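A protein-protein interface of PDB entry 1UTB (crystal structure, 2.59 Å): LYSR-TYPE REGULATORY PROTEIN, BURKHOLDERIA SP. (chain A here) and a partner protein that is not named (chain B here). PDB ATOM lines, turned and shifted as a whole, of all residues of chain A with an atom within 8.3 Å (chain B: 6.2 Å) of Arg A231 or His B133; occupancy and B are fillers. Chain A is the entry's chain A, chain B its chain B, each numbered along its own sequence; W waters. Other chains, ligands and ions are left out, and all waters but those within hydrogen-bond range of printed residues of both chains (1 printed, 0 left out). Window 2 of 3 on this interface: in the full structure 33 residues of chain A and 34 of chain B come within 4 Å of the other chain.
Arg A231 touches just these residues of chain B: Met B124, Leu B127, Ala B128, Ala B131, Pro B132, His B133, Ile B134, Gln B135 and Ile B136.
His B133 touches just one residue of chain A: Arg A231 (3.9 Å).
Of the printed residues of chain A, Ser B137 touches Val A233 (3.3 Å).
Of the printed residues of chain A, Ile B134 touches Arg A231.
Of the printed residues of chain B, Leu A232 touches Met B124 (3.8 Å) and Ile B136 (3.2 Å).
Of the printed residues of chain B, Val A233 touches Ile B136 (3.0 Å) and Ser B137 (3.3 Å).
Gln B129 touches none of the printed residues of chain A.
Thr B104 touches none of the printed residues of chain A.
Hydrophobic or aromatic side chains of chain A that line the printed part of chain B: Leu A232.
Among the printed residues, no Asp or Glu carboxylate lies within 4 Å of a Lys or Arg side-chain nitrogen of the other chain.
The backbone carbonyl oxygen (O) of Met A230 sits close to the side-chain amide oxygen (OE1) of Gln B135 (3.0 Å).
The guanidinium group (NH1) of Arg A231 lies within hydrogen-bond range of the backbone carbonyl oxygen (O) of Leu B127 (3.4 Å).
O of Ala B131 sits at hydrogen-bond distance from NH2 of Arg A231, at 2.4 Å.
The backbone carbonyl oxygen (O) of Ile B134 is in hydrogen-bond range of the guanidinium group (NE) of Arg A231 (3.3 Å).
The backbone NH (N) of Ile B136 lies within hydrogen-bond range of the backbone carbonyl oxygen (O) of Arg A231 (2.9 Å).
The backbone NH (N) of Val A233 lies within hydrogen-bond range of the backbone carbonyl oxygen (O) of Ile B136, 3.0 Å away.
Among the printed residues, pairs that only touch across the chains: Leu A232 with Ile B136 (3.2 Å), Val A233 with Ser B137 (3.3 Å), Arg A231 with Pro B132 (3.5 Å), Arg A231 with Gln B135 (3.6 Å), Arg A231 with Ala B128 (3.6 Å), Glu A203 with Pro B132 (3.7 Å), Thr A247 with Met B124 (3.8 Å), Leu A232 with Met B124 (3.8 Å), Arg A231 with Met B124 (3.8 Å) and Arg A231 with His B133 (3.9 Å).
The side-chain carboxylate (OE2) of Glu A203 is in salt-bridge range of the guanidinium group (NH2) of Arg A229 (3.7 Å).
The backbone NH (N) of Arg A231 lies within hydrogen-bond range of the backbone carbonyl oxygen (O) of His A204, at 3.1 Å.
The backbone carbonyl oxygen of His A204 lies within hydrogen-bond range of the backbone NH of Leu A232, at 3.3 Å.
N of Gly A206 sits at hydrogen-bond distance from O of Leu A232.
The side-chain sulfur (SD) of Met A230 sits close to the guanidinium group (NE) of Arg A228 (3.7 Å).
N of Gln B135 is in hydrogen-bond range of O of Arg B105, 3.0 Å away.
Water W1 lies within hydrogen-bond range of the backbone carbonyl oxygen of Met A230 and the backbone carbonyl oxygen of Ile B136.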
ATOM      1  N   LEU A 202     -19.373 -12.655   5.460  1.00  0.00           N
ATOM      2  CA  LEU A 202     -20.104 -12.361   4.243  1.00  0.00           C
ATOM      3  C   LEU A 202     -19.717 -13.322   3.127  1.00  0.00           C
ATOM      4  O   LEU A 202     -18.702 -14.002   3.191  1.00  0.00           O
ATOM      5  CB  LEU A 202     -19.794 -10.939   3.814  1.00  0.00           C
ATOM      6  CG  LEU A 202     -20.818  -9.831   4.031  1.00  0.00           C
ATOM      7  CD1 LEU A 202     -21.868 -10.155   5.053  1.00  0.00           C
ATOM      8  CD2 LEU A 202     -20.068  -8.552   4.370  1.00  0.00           C
ATOM      9  N   GLU A 203     -20.552 -13.377   2.103  1.00  0.00           N
ATOM     10  CA  GLU A 203     -20.260 -14.202   0.932  1.00  0.00           C
ATOM     11  C   GLU A 203     -19.554 -13.433  -0.183  1.00  0.00           C
ATOM     12  O   GLU A 203     -19.812 -12.259  -0.391  1.00  0.00           O
ATOM     13  CB  GLU A 203     -21.545 -14.802   0.398  1.00  0.00           C
ATOM     14  CG  GLU A 203     -22.025 -15.996   1.196  1.00  0.00           C
ATOM     15  CD  GLU A 203     -23.378 -16.449   0.733  1.00  0.00           C
ATOM     16  OE1 GLU A 203     -24.239 -15.565   0.503  1.00  0.00           O
ATOM     17  OE2 GLU A 203     -23.550 -17.675   0.548  1.00  0.00           O
ATOM     18  N   HIS A 204     -18.685 -14.135  -0.906  1.00  0.00           N
ATOM     19  CA  HIS A 204     -17.803 -13.514  -1.887  1.00  0.00           C
ATOM     20  C   HIS A 204     -17.904 -14.059  -3.295  1.00  0.00           C
ATOM     21  O   HIS A 204     -18.218 -15.221  -3.494  1.00  0.00           O
ATOM     22  CB  HIS A 204     -16.357 -13.714  -1.490  1.00  0.00           C
ATOM     23  CG  HIS A 204     -16.024 -13.207  -0.131  1.00  0.00           C
ATOM     24  ND1 HIS A 204     -14.968 -12.357   0.099  1.00  0.00           N
ATOM     25  CD2 HIS A 204     -16.581 -13.454   1.074  1.00  0.00           C
ATOM     26  CE1 HIS A 204     -14.894 -12.100   1.393  1.00  0.00           C
ATOM     27  NE2 HIS A 204     -15.862 -12.755   2.006  1.00  0.00           N
ATOM     28  N   VAL A 205     -17.608 -13.172  -4.251  1.00  0.00           N
ATOM     29  CA  VAL A 205     -17.195 -13.512  -5.614  1.00  0.00           C
ATOM     30  C   VAL A 205     -15.695 -13.356  -5.631  1.00  0.00           C
ATOM     31  O   VAL A 205     -15.186 -12.270  -5.345  1.00  0.00           O
ATOM     32  CB  VAL A 205     -17.653 -12.498  -6.696  1.00  0.00           C
ATOM     33  CG1 VAL A 205     -18.208 -13.211  -7.888  1.00  0.00           C
ATOM     34  CG2 VAL A 205     -18.618 -11.447  -6.177  1.00  0.00           C
ATOM     35  N   GLY A 206     -14.987 -14.418  -5.975  1.00  0.00           N
ATOM     36  CA  GLY A 206     -13.563 -14.340  -6.205  1.00  0.00           C
ATOM     37  C   GLY A 206     -13.312 -14.289  -7.697  1.00  0.00           C
ATOM     38  O   GLY A 206     -14.122 -14.810  -8.462  1.00  0.00           O
ATOM     39  N   ARG A 228     -12.944 -17.592   3.841  1.00  0.00           N
ATOM     40  CA  ARG A 228     -13.822 -16.918   2.902  1.00  0.00           C
ATOM     41  C   ARG A 228     -14.823 -17.902   2.331  1.00  0.00           C
ATOM     42  O   ARG A 228     -14.450 -18.964   1.843  1.00  0.00           O
ATOM     43  CB  ARG A 228     -12.981 -16.300   1.793  1.00  0.00           C
ATOM     44  CG  ARG A 228     -13.402 -14.919   1.396  1.00  0.00           C
ATOM     45  CD  ARG A 228     -12.295 -14.081   0.804  1.00  0.00           C
ATOM     46  NE  ARG A 228     -11.329 -14.872   0.052  1.00  0.00           N
ATOM     47  CZ  ARG A 228     -11.020 -14.685  -1.225  1.00  0.00           C
ATOM     48  NH1 ARG A 228     -11.599 -13.724  -1.946  1.00  0.00           N
ATOM     49  NH2 ARG A 228     -10.110 -15.478  -1.793  1.00  0.00           N
ATOM     50  N   ARG A 229     -16.092 -17.538   2.437  1.00  0.00           N
ATOM     51  CA  ARG A 229     -17.196 -18.255   1.828  1.00  0.00           C
ATOM     52  C   ARG A 229     -17.277 -17.882   0.338  1.00  0.00           C
ATOM     53  O   ARG A 229     -17.834 -16.842  -0.018  1.00  0.00           O
ATOM     54  CB  ARG A 229     -18.504 -17.907   2.553  1.00  0.00           C
ATOM     55  CG  ARG A 229     -18.706 -18.687   3.874  1.00  0.00           C
ATOM     56  CD  ARG A 229     -19.377 -17.917   5.056  1.00  0.00           C
ATOM     57  NE  ARG A 229     -20.625 -17.207   4.732  1.00  0.00           N
ATOM     58  CZ  ARG A 229     -21.785 -17.790   4.417  1.00  0.00           C
ATOM     59  NH1 ARG A 229     -21.881 -19.113   4.339  1.00  0.00           N
ATOM     60  NH2 ARG A 229     -22.860 -17.046   4.152  1.00  0.00           N
ATOM     61  N   MET A 230     -16.696 -18.730  -0.515  1.00  0.00           N
ATOM     62  CA  MET A 230     -16.595 -18.467  -1.946  1.00  0.00           C
ATOM     63  C   MET A 230     -17.809 -19.036  -2.648  1.00  0.00           C
ATOM     64  O   MET A 230     -17.809 -20.192  -3.072  1.00  0.00           O
ATOM     65  CB  MET A 230     -15.322 -19.092  -2.531  1.00  0.00           C
ATOM     66  CG  MET A 230     -14.003 -18.597  -1.922  1.00  0.00           C
ATOM     67  SD  MET A 230     -13.751 -16.787  -1.964  1.00  0.00           S
ATOM     68  CE  MET A 230     -14.222 -16.411  -3.633  1.00  0.00           C
ATOM     69  N   ARG A 231     -18.847 -18.211  -2.738  1.00  0.00           N
ATOM     70  CA  ARG A 231     -20.060 -18.532  -3.461  1.00  0.00           C
ATOM     71  C   ARG A 231     -19.869 -18.635  -4.956  1.00  0.00           C
ATOM     72  O   ARG A 231     -20.433 -19.516  -5.580  1.00  0.00           O
ATOM     73  CB  ARG A 231     -21.117 -17.458  -3.235  1.00  0.00           C
ATOM     74  CG  ARG A 231     -22.231 -17.908  -2.380  1.00  0.00           C
ATOM     75  CD  ARG A 231     -23.591 -17.863  -3.013  1.00  0.00           C
ATOM     76  NE  ARG A 231     -24.157 -19.199  -3.186  1.00  0.00           N
ATOM     77  CZ  ARG A 231     -25.452 -19.443  -3.385  1.00  0.00           C
ATOM     78  NH1 ARG A 231     -26.349 -18.465  -3.411  1.00  0.00           N
ATOM     79  NH2 ARG A 231     -25.853 -20.678  -3.563  1.00  0.00           N
ATOM     80  N   LEU A 232     -19.145 -17.683  -5.530  1.00  0.00           N
ATOM     81  CA  LEU A 232     -18.904 -17.629  -6.958  1.00  0.00           C
ATOM     82  C   LEU A 232     -17.448 -17.362  -7.189  1.00  0.00           C
ATOM     83  O   LEU A 232     -16.911 -16.434  -6.619  1.00  0.00           O
ATOM     84  CB  LEU A 232     -19.712 -16.502  -7.588  1.00  0.00           C
ATOM     85  CG  LEU A 232     -20.174 -16.577  -9.050  1.00  0.00           C
ATOM     86  CD1 LEU A 232     -19.970 -15.242  -9.729  1.00  0.00           C
ATOM     87  CD2 LEU A 232     -19.532 -17.702  -9.845  1.00  0.00           C
ATOM     88  N   VAL A 233     -16.813 -18.204  -8.002  1.00  0.00           N
ATOM     89  CA  VAL A 233     -15.479 -17.950  -8.544  1.00  0.00           C
ATOM     90  C   VAL A 233     -15.605 -17.785 -10.061  1.00  0.00           C
ATOM     91  O   VAL A 233     -16.272 -18.567 -10.721  1.00  0.00           O
ATOM     92  CB  VAL A 233     -14.493 -19.088  -8.201  1.00  0.00           C
ATOM     93  CG1 VAL A 233     -13.132 -18.877  -8.891  1.00  0.00           C
ATOM     94  CG2 VAL A 233     -14.300 -19.158  -6.704  1.00  0.00           C
ATOM     95  N   VAL A 234     -14.994 -16.730 -10.587  1.00  0.00           N
ATOM     96  CA  VAL A 234     -14.940 -16.455 -12.020  1.00  0.00           C
ATOM     97  C   VAL A 234     -13.480 -16.269 -12.424  1.00  0.00           C
ATOM     98  O   VAL A 234     -12.656 -15.928 -11.589  1.00  0.00           O
ATOM     99  CB  VAL A 234     -15.746 -15.210 -12.382  1.00  0.00           C
ATOM    100  CG1 VAL A 234     -17.198 -15.435 -12.111  1.00  0.00           C
ATOM    101  CG2 VAL A 234     -15.246 -13.980 -11.659  1.00  0.00           C
ATOM    102  N   THR A 247     -26.596  -8.834  -6.289  1.00  0.00           N
ATOM    103  CA  THR A 247     -26.466  -9.751  -5.172  1.00  0.00           C
ATOM    104  C   THR A 247     -25.956  -9.039  -3.926  1.00  0.00           C
ATOM    105  O   THR A 247     -25.685  -7.839  -3.944  1.00  0.00           O
ATOM    106  CB  THR A 247     -25.518 -10.909  -5.528  1.00  0.00           C
ATOM    107  OG1 THR A 247     -24.217 -10.398  -5.839  1.00  0.00           O
ATOM    108  CG2 THR A 247     -25.957 -11.598  -6.783  1.00  0.00           C
ATOM    109  N   ASP A 248     -25.848  -9.797  -2.842  1.00  0.00           N
ATOM    110  CA  ASP A 248     -25.262  -9.317  -1.597  1.00  0.00           C
ATOM    111  C   ASP A 248     -23.834  -9.842  -1.453  1.00  0.00           C
ATOM    112  O   ASP A 248     -23.282  -9.912  -0.356  1.00  0.00           O
ATOM    113  CB  ASP A 248     -26.128  -9.764  -0.417  1.00  0.00           C
ATOM    114  CG  ASP A 248     -27.498  -9.092  -0.408  1.00  0.00           C
ATOM    115  OD1 ASP A 248     -28.428  -9.622   0.252  1.00  0.00           O
ATOM    116  OD2 ASP A 248     -27.734  -8.037  -1.026  1.00  0.00           O
ATOM    117  N   LEU A 249     -23.240 -10.218  -2.580  1.00  0.00           N
ATOM    118  CA  LEU A 249     -21.869 -10.702  -2.611  1.00  0.00           C
ATOM    119  C   LEU A 249     -20.956  -9.509  -2.455  1.00  0.00           C
ATOM    120  O   LEU A 249     -21.332  -8.369  -2.743  1.00  0.00           O
ATOM    121  CB  LEU A 249     -21.560 -11.377  -3.946  1.00  0.00           C
ATOM    122  CG  LEU A 249     -21.656 -12.890  -4.169  1.00  0.00           C
ATOM    123  CD1 LEU A 249     -22.232 -13.639  -3.010  1.00  0.00           C
ATOM    124  CD2 LEU A 249     -22.434 -13.176  -5.455  1.00  0.00           C
ATOM    125  N   ILE A 250     -19.751  -9.786  -1.998  1.00  0.00           N
ATOM    126  CA  ILE A 250     -18.700  -8.787  -1.928  1.00  0.00           C
ATOM    127  C   ILE A 250     -17.483  -9.306  -2.696  1.00  0.00           C
ATOM    128  O   ILE A 250     -17.276 -10.517  -2.810  1.00  0.00           O
ATOM    129  CB  ILE A 250     -18.357  -8.441  -0.445  1.00  0.00           C
ATOM    130  CG1 ILE A 250     -17.641  -9.581   0.253  1.00  0.00           C
ATOM    131  CG2 ILE A 250     -19.630  -8.091   0.364  1.00  0.00           C
ATOM    132  CD1 ILE A 250     -17.041  -9.152   1.577  1.00  0.00           C
ATOM    133  N   PRO B 100     -31.703 -28.935  -2.957  1.00  0.00           N
ATOM    134  CA  PRO B 100     -31.198 -27.578  -3.185  1.00  0.00           C
ATOM    135  C   PRO B 100     -30.979 -26.766  -1.916  1.00  0.00           C
ATOM    136  O   PRO B 100     -30.013 -26.015  -1.860  1.00  0.00           O
ATOM    137  CB  PRO B 100     -32.279 -26.941  -4.068  1.00  0.00           C
ATOM    138  CG  PRO B 100     -33.453 -27.797  -3.914  1.00  0.00           C
ATOM    139  CD  PRO B 100     -32.948 -29.181  -3.705  1.00  0.00           C
ATOM    140  N   PHE B 101     -31.843 -26.915  -0.921  1.00  0.00           N
ATOM    141  CA  PHE B 101     -31.719 -26.170   0.334  1.00  0.00           C
ATOM    142  C   PHE B 101     -30.487 -26.578   1.147  1.00  0.00           C
ATOM    143  O   PHE B 101     -29.906 -25.748   1.837  1.00  0.00           O
ATOM    144  CB  PHE B 101     -32.965 -26.351   1.203  1.00  0.00           C
ATOM    145  CG  PHE B 101     -34.235 -25.769   0.619  1.00  0.00           C
ATOM    146  CD1 PHE B 101     -35.430 -25.852   1.340  1.00  0.00           C
ATOM    147  CD2 PHE B 101     -34.261 -25.147  -0.643  1.00  0.00           C
ATOM    148  CE1 PHE B 101     -36.612 -25.324   0.830  1.00  0.00           C
ATOM    149  CE2 PHE B 101     -35.450 -24.618  -1.155  1.00  0.00           C
ATOM    150  CZ  PHE B 101     -36.626 -24.704  -0.416  1.00  0.00           C
ATOM    151  N   ALA B 102     -30.099 -27.846   1.067  1.00  0.00           N
ATOM    152  CA  ALA B 102     -28.991 -28.369   1.870  1.00  0.00           C
ATOM    153  C   ALA B 102     -27.682 -28.544   1.109  1.00  0.00           C
ATOM    154  O   ALA B 102     -26.614 -28.450   1.705  1.00  0.00           O
ATOM    155  CB  ALA B 102     -29.397 -29.693   2.524  1.00  0.00           C
ATOM    156  N   SER B 103     -27.764 -28.789  -0.199  1.00  0.00           N
ATOM    157  CA  SER B 103     -26.583 -29.104  -1.002  1.00  0.00           C
ATOM    158  C   SER B 103     -25.492 -28.074  -0.883  1.00  0.00           C
ATOM    159  O   SER B 103     -25.732 -26.874  -0.869  1.00  0.00           O
ATOM    160  CB  SER B 103     -26.893 -29.299  -2.486  1.00  0.00           C
ATOM    161  OG  SER B 103     -25.710 -29.705  -3.171  1.00  0.00           O
ATOM    162  N   THR B 104     -24.282 -28.596  -0.837  1.00  0.00           N
ATOM    163  CA  THR B 104     -23.079 -27.860  -0.541  1.00  0.00           C
ATOM    164  C   THR B 104     -22.079 -28.027  -1.709  1.00  0.00           C
ATOM    165  O   THR B 104     -20.907 -27.606  -1.654  1.00  0.00           O
ATOM    166  CB  THR B 104     -22.565 -28.418   0.816  1.00  0.00           C
ATOM    167  OG1 THR B 104     -22.191 -27.333   1.664  1.00  0.00           O
ATOM    168  CG2 THR B 104     -21.325 -29.341   0.697  1.00  0.00           C
ATOM    169  N   ARG B 105     -22.591 -28.591  -2.795  1.00  0.00           N
ATOM    170  CA  ARG B 105     -21.762 -29.022  -3.904  1.00  0.00           C
ATOM    171  C   ARG B 105     -21.415 -27.835  -4.811  1.00  0.00           C
ATOM    172  O   ARG B 105     -22.139 -26.834  -4.867  1.00  0.00           O
ATOM    173  CB  ARG B 105     -22.478 -30.157  -4.645  1.00  0.00           C
ATOM    174  CG  ARG B 105     -22.554 -30.053  -6.140  1.00  0.00           C
ATOM    175  CD  ARG B 105     -23.396 -31.146  -6.751  1.00  0.00           C
ATOM    176  NE  ARG B 105     -23.102 -31.334  -8.173  1.00  0.00           N
ATOM    177  CZ  ARG B 105     -23.746 -32.199  -8.951  1.00  0.00           C
ATOM    178  NH1 ARG B 105     -24.729 -32.948  -8.467  1.00  0.00           N
ATOM    179  NH2 ARG B 105     -23.410 -32.303 -10.232  1.00  0.00           N
ATOM    180  N   MET B 124     -26.995 -15.932  -9.935  1.00  0.00           N
ATOM    181  CA  MET B 124     -26.607 -15.802  -8.534  1.00  0.00           C
ATOM    182  C   MET B 124     -27.741 -15.208  -7.696  1.00  0.00           C
ATOM    183  O   MET B 124     -27.985 -15.652  -6.588  1.00  0.00           O
ATOM    184  CB  MET B 124     -25.331 -14.977  -8.397  1.00  0.00           C
ATOM    185  CG  MET B 124     -24.102 -15.650  -8.968  1.00  0.00           C
ATOM    186  SD  MET B 124     -23.862 -17.381  -8.554  1.00  0.00           S
ATOM    187  CE  MET B 124     -23.821 -17.234  -6.762  1.00  0.00           C
ATOM    188  N   LEU B 127     -30.104 -18.118  -7.149  1.00  0.00           N
ATOM    189  CA  LEU B 127     -29.553 -19.146  -6.275  1.00  0.00           C
ATOM    190  C   LEU B 127     -29.544 -18.705  -4.813  1.00  0.00           C
ATOM    191  O   LEU B 127     -29.494 -19.533  -3.922  1.00  0.00           O
ATOM    192  CB  LEU B 127     -28.127 -19.498  -6.700  1.00  0.00           C
ATOM    193  CG  LEU B 127     -27.947 -20.340  -7.954  1.00  0.00           C
ATOM    194  CD1 LEU B 127     -26.475 -20.517  -8.249  1.00  0.00           C
ATOM    195  CD2 LEU B 127     -28.613 -21.683  -7.798  1.00  0.00           C
ATOM    196  N   ALA B 128     -29.566 -17.397  -4.576  1.00  0.00           N
ATOM    197  CA  ALA B 128     -29.559 -16.852  -3.224  1.00  0.00           C
ATOM    198  C   ALA B 128     -30.810 -17.324  -2.500  1.00  0.00           C
ATOM    199  O   ALA B 128     -30.773 -17.599  -1.294  1.00  0.00           O
ATOM    200  CB  ALA B 128     -29.510 -15.332  -3.244  1.00  0.00           C
ATOM    201  N   GLN B 129     -31.900 -17.452  -3.258  1.00  0.00           N
ATOM    202  CA  GLN B 129     -33.184 -17.871  -2.709  1.00  0.00           C
ATOM    203  C   GLN B 129     -33.475 -19.359  -2.896  1.00  0.00           C
ATOM    204  O   GLN B 129     -34.368 -19.863  -2.259  1.00  0.00           O
ATOM    205  CB  GLN B 129     -34.326 -17.042  -3.308  1.00  0.00           C
ATOM    206  CG  GLN B 129     -33.985 -15.545  -3.627  1.00  0.00           C
ATOM    207  CD  GLN B 129     -33.623 -14.691  -2.379  1.00  0.00           C
ATOM    208  OE1 GLN B 129     -34.059 -14.985  -1.249  1.00  0.00           O
ATOM    209  NE2 GLN B 129     -32.823 -13.633  -2.598  1.00  0.00           N
ATOM    210  N   ALA B 131     -30.838 -22.208  -3.634  1.00  0.00           N
ATOM    211  CA  ALA B 131     -29.833 -23.136  -3.163  1.00  0.00           C
ATOM    212  C   ALA B 131     -28.712 -22.362  -2.483  1.00  0.00           C
ATOM    213  O   ALA B 131     -27.667 -22.215  -3.061  1.00  0.00           O
ATOM    214  CB  ALA B 131     -29.302 -23.966  -4.343  1.00  0.00           C
ATOM    215  N   PRO B 132     -28.937 -21.872  -1.257  1.00  0.00           N
ATOM    216  CA  PRO B 132     -28.027 -20.904  -0.594  1.00  0.00           C
ATOM    217  C   PRO B 132     -26.613 -21.387  -0.226  1.00  0.00           C
ATOM    218  O   PRO B 132     -25.784 -20.545   0.108  1.00  0.00           O
ATOM    219  CB  PRO B 132     -28.782 -20.537   0.693  1.00  0.00           C
ATOM    220  CG  PRO B 132     -30.174 -20.997   0.476  1.00  0.00           C
ATOM    221  CD  PRO B 132     -30.102 -22.192  -0.408  1.00  0.00           C
ATOM    222  N   HIS B 133     -26.356 -22.693  -0.294  1.00  0.00           N
ATOM    223  CA  HIS B 133     -25.079 -23.260   0.121  1.00  0.00           C
ATOM    224  C   HIS B 133     -24.297 -23.918  -0.995  1.00  0.00           C
ATOM    225  O   HIS B 133     -23.246 -24.498  -0.729  1.00  0.00           O
ATOM    226  CB  HIS B 133     -25.290 -24.287   1.245  1.00  0.00           C
ATOM    227  CG  HIS B 133     -26.026 -23.728   2.413  1.00  0.00           C
ATOM    228  ND1 HIS B 133     -27.285 -24.156   2.772  1.00  0.00           N
ATOM    229  CD2 HIS B 133     -25.709 -22.723   3.264  1.00  0.00           C
ATOM    230  CE1 HIS B 133     -27.706 -23.452   3.807  1.00  0.00           C
ATOM    231  NE2 HIS B 133     -26.771 -22.573   4.125  1.00  0.00           N
ATOM    232  N   ILE B 134     -24.779 -23.872  -2.235  1.00  0.00           N
ATOM    233  CA  ILE B 134     -23.965 -24.423  -3.316  1.00  0.00           C
ATOM    234  C   ILE B 134     -22.896 -23.413  -3.687  1.00  0.00           C
ATOM    235  O   ILE B 134     -22.982 -22.250  -3.349  1.00  0.00           O
ATOM    236  CB  ILE B 134     -24.809 -24.878  -4.553  1.00  0.00           C
ATOM    237  CG1 ILE B 134     -25.626 -23.736  -5.166  1.00  0.00           C
ATOM    238  CG2 ILE B 134     -25.724 -26.034  -4.178  1.00  0.00           C
ATOM    239  CD1 ILE B 134     -26.049 -24.026  -6.587  1.00  0.00           C
ATOM    240  N   GLN B 135     -21.863 -23.881  -4.348  1.00  0.00           N
ATOM    241  CA  GLN B 135     -20.850 -22.995  -4.897  1.00  0.00           C
ATOM    242  C   GLN B 135     -20.869 -23.101  -6.414  1.00  0.00           C
ATOM    243  O   GLN B 135     -20.999 -24.188  -6.955  1.00  0.00           O
ATOM    244  CB  GLN B 135     -19.478 -23.360  -4.341  1.00  0.00           C
ATOM    245  CG  GLN B 135     -19.452 -23.423  -2.788  1.00  0.00           C
ATOM    246  CD  GLN B 135     -18.111 -23.817  -2.261  1.00  0.00           C
ATOM    247  OE1 GLN B 135     -17.187 -23.016  -2.302  1.00  0.00           O
ATOM    248  NE2 GLN B 135     -17.980 -25.067  -1.798  1.00  0.00           N
ATOM    249  N   ILE B 136     -20.788 -21.957  -7.082  1.00  0.00           N
ATOM    250  CA  ILE B 136     -20.630 -21.908  -8.513  1.00  0.00           C
ATOM    251  C   ILE B 136     -19.238 -21.445  -8.862  1.00  0.00           C
ATOM    252  O   ILE B 136     -18.697 -20.537  -8.257  1.00  0.00           O
ATOM    253  CB  ILE B 136     -21.630 -20.958  -9.131  1.00  0.00           C
ATOM    254  CG1 ILE B 136     -23.063 -21.358  -8.771  1.00  0.00           C
ATOM    255  CG2 ILE B 136     -21.448 -20.934 -10.648  1.00  0.00           C
ATOM    256  CD1 ILE B 136     -23.444 -22.743  -9.206  1.00  0.00           C
ATOM    257  N   SER B 137     -18.657 -22.077  -9.863  1.00  0.00           N
ATOM    258  CA  SER B 137     -17.390 -21.629 -10.401  1.00  0.00           C
ATOM    259  C   SER B 137     -17.455 -21.670 -11.933  1.00  0.00           C
ATOM    260  O   SER B 137     -17.918 -22.637 -12.487  1.00  0.00           O
ATOM    261  CB  SER B 137     -16.273 -22.484  -9.816  1.00  0.00           C
ATOM    262  OG  SER B 137     -15.439 -22.991 -10.816  1.00  0.00           O
HETATM  263  O   HOH W   1     -17.145 -21.000  -5.670  1.00  0.00           O
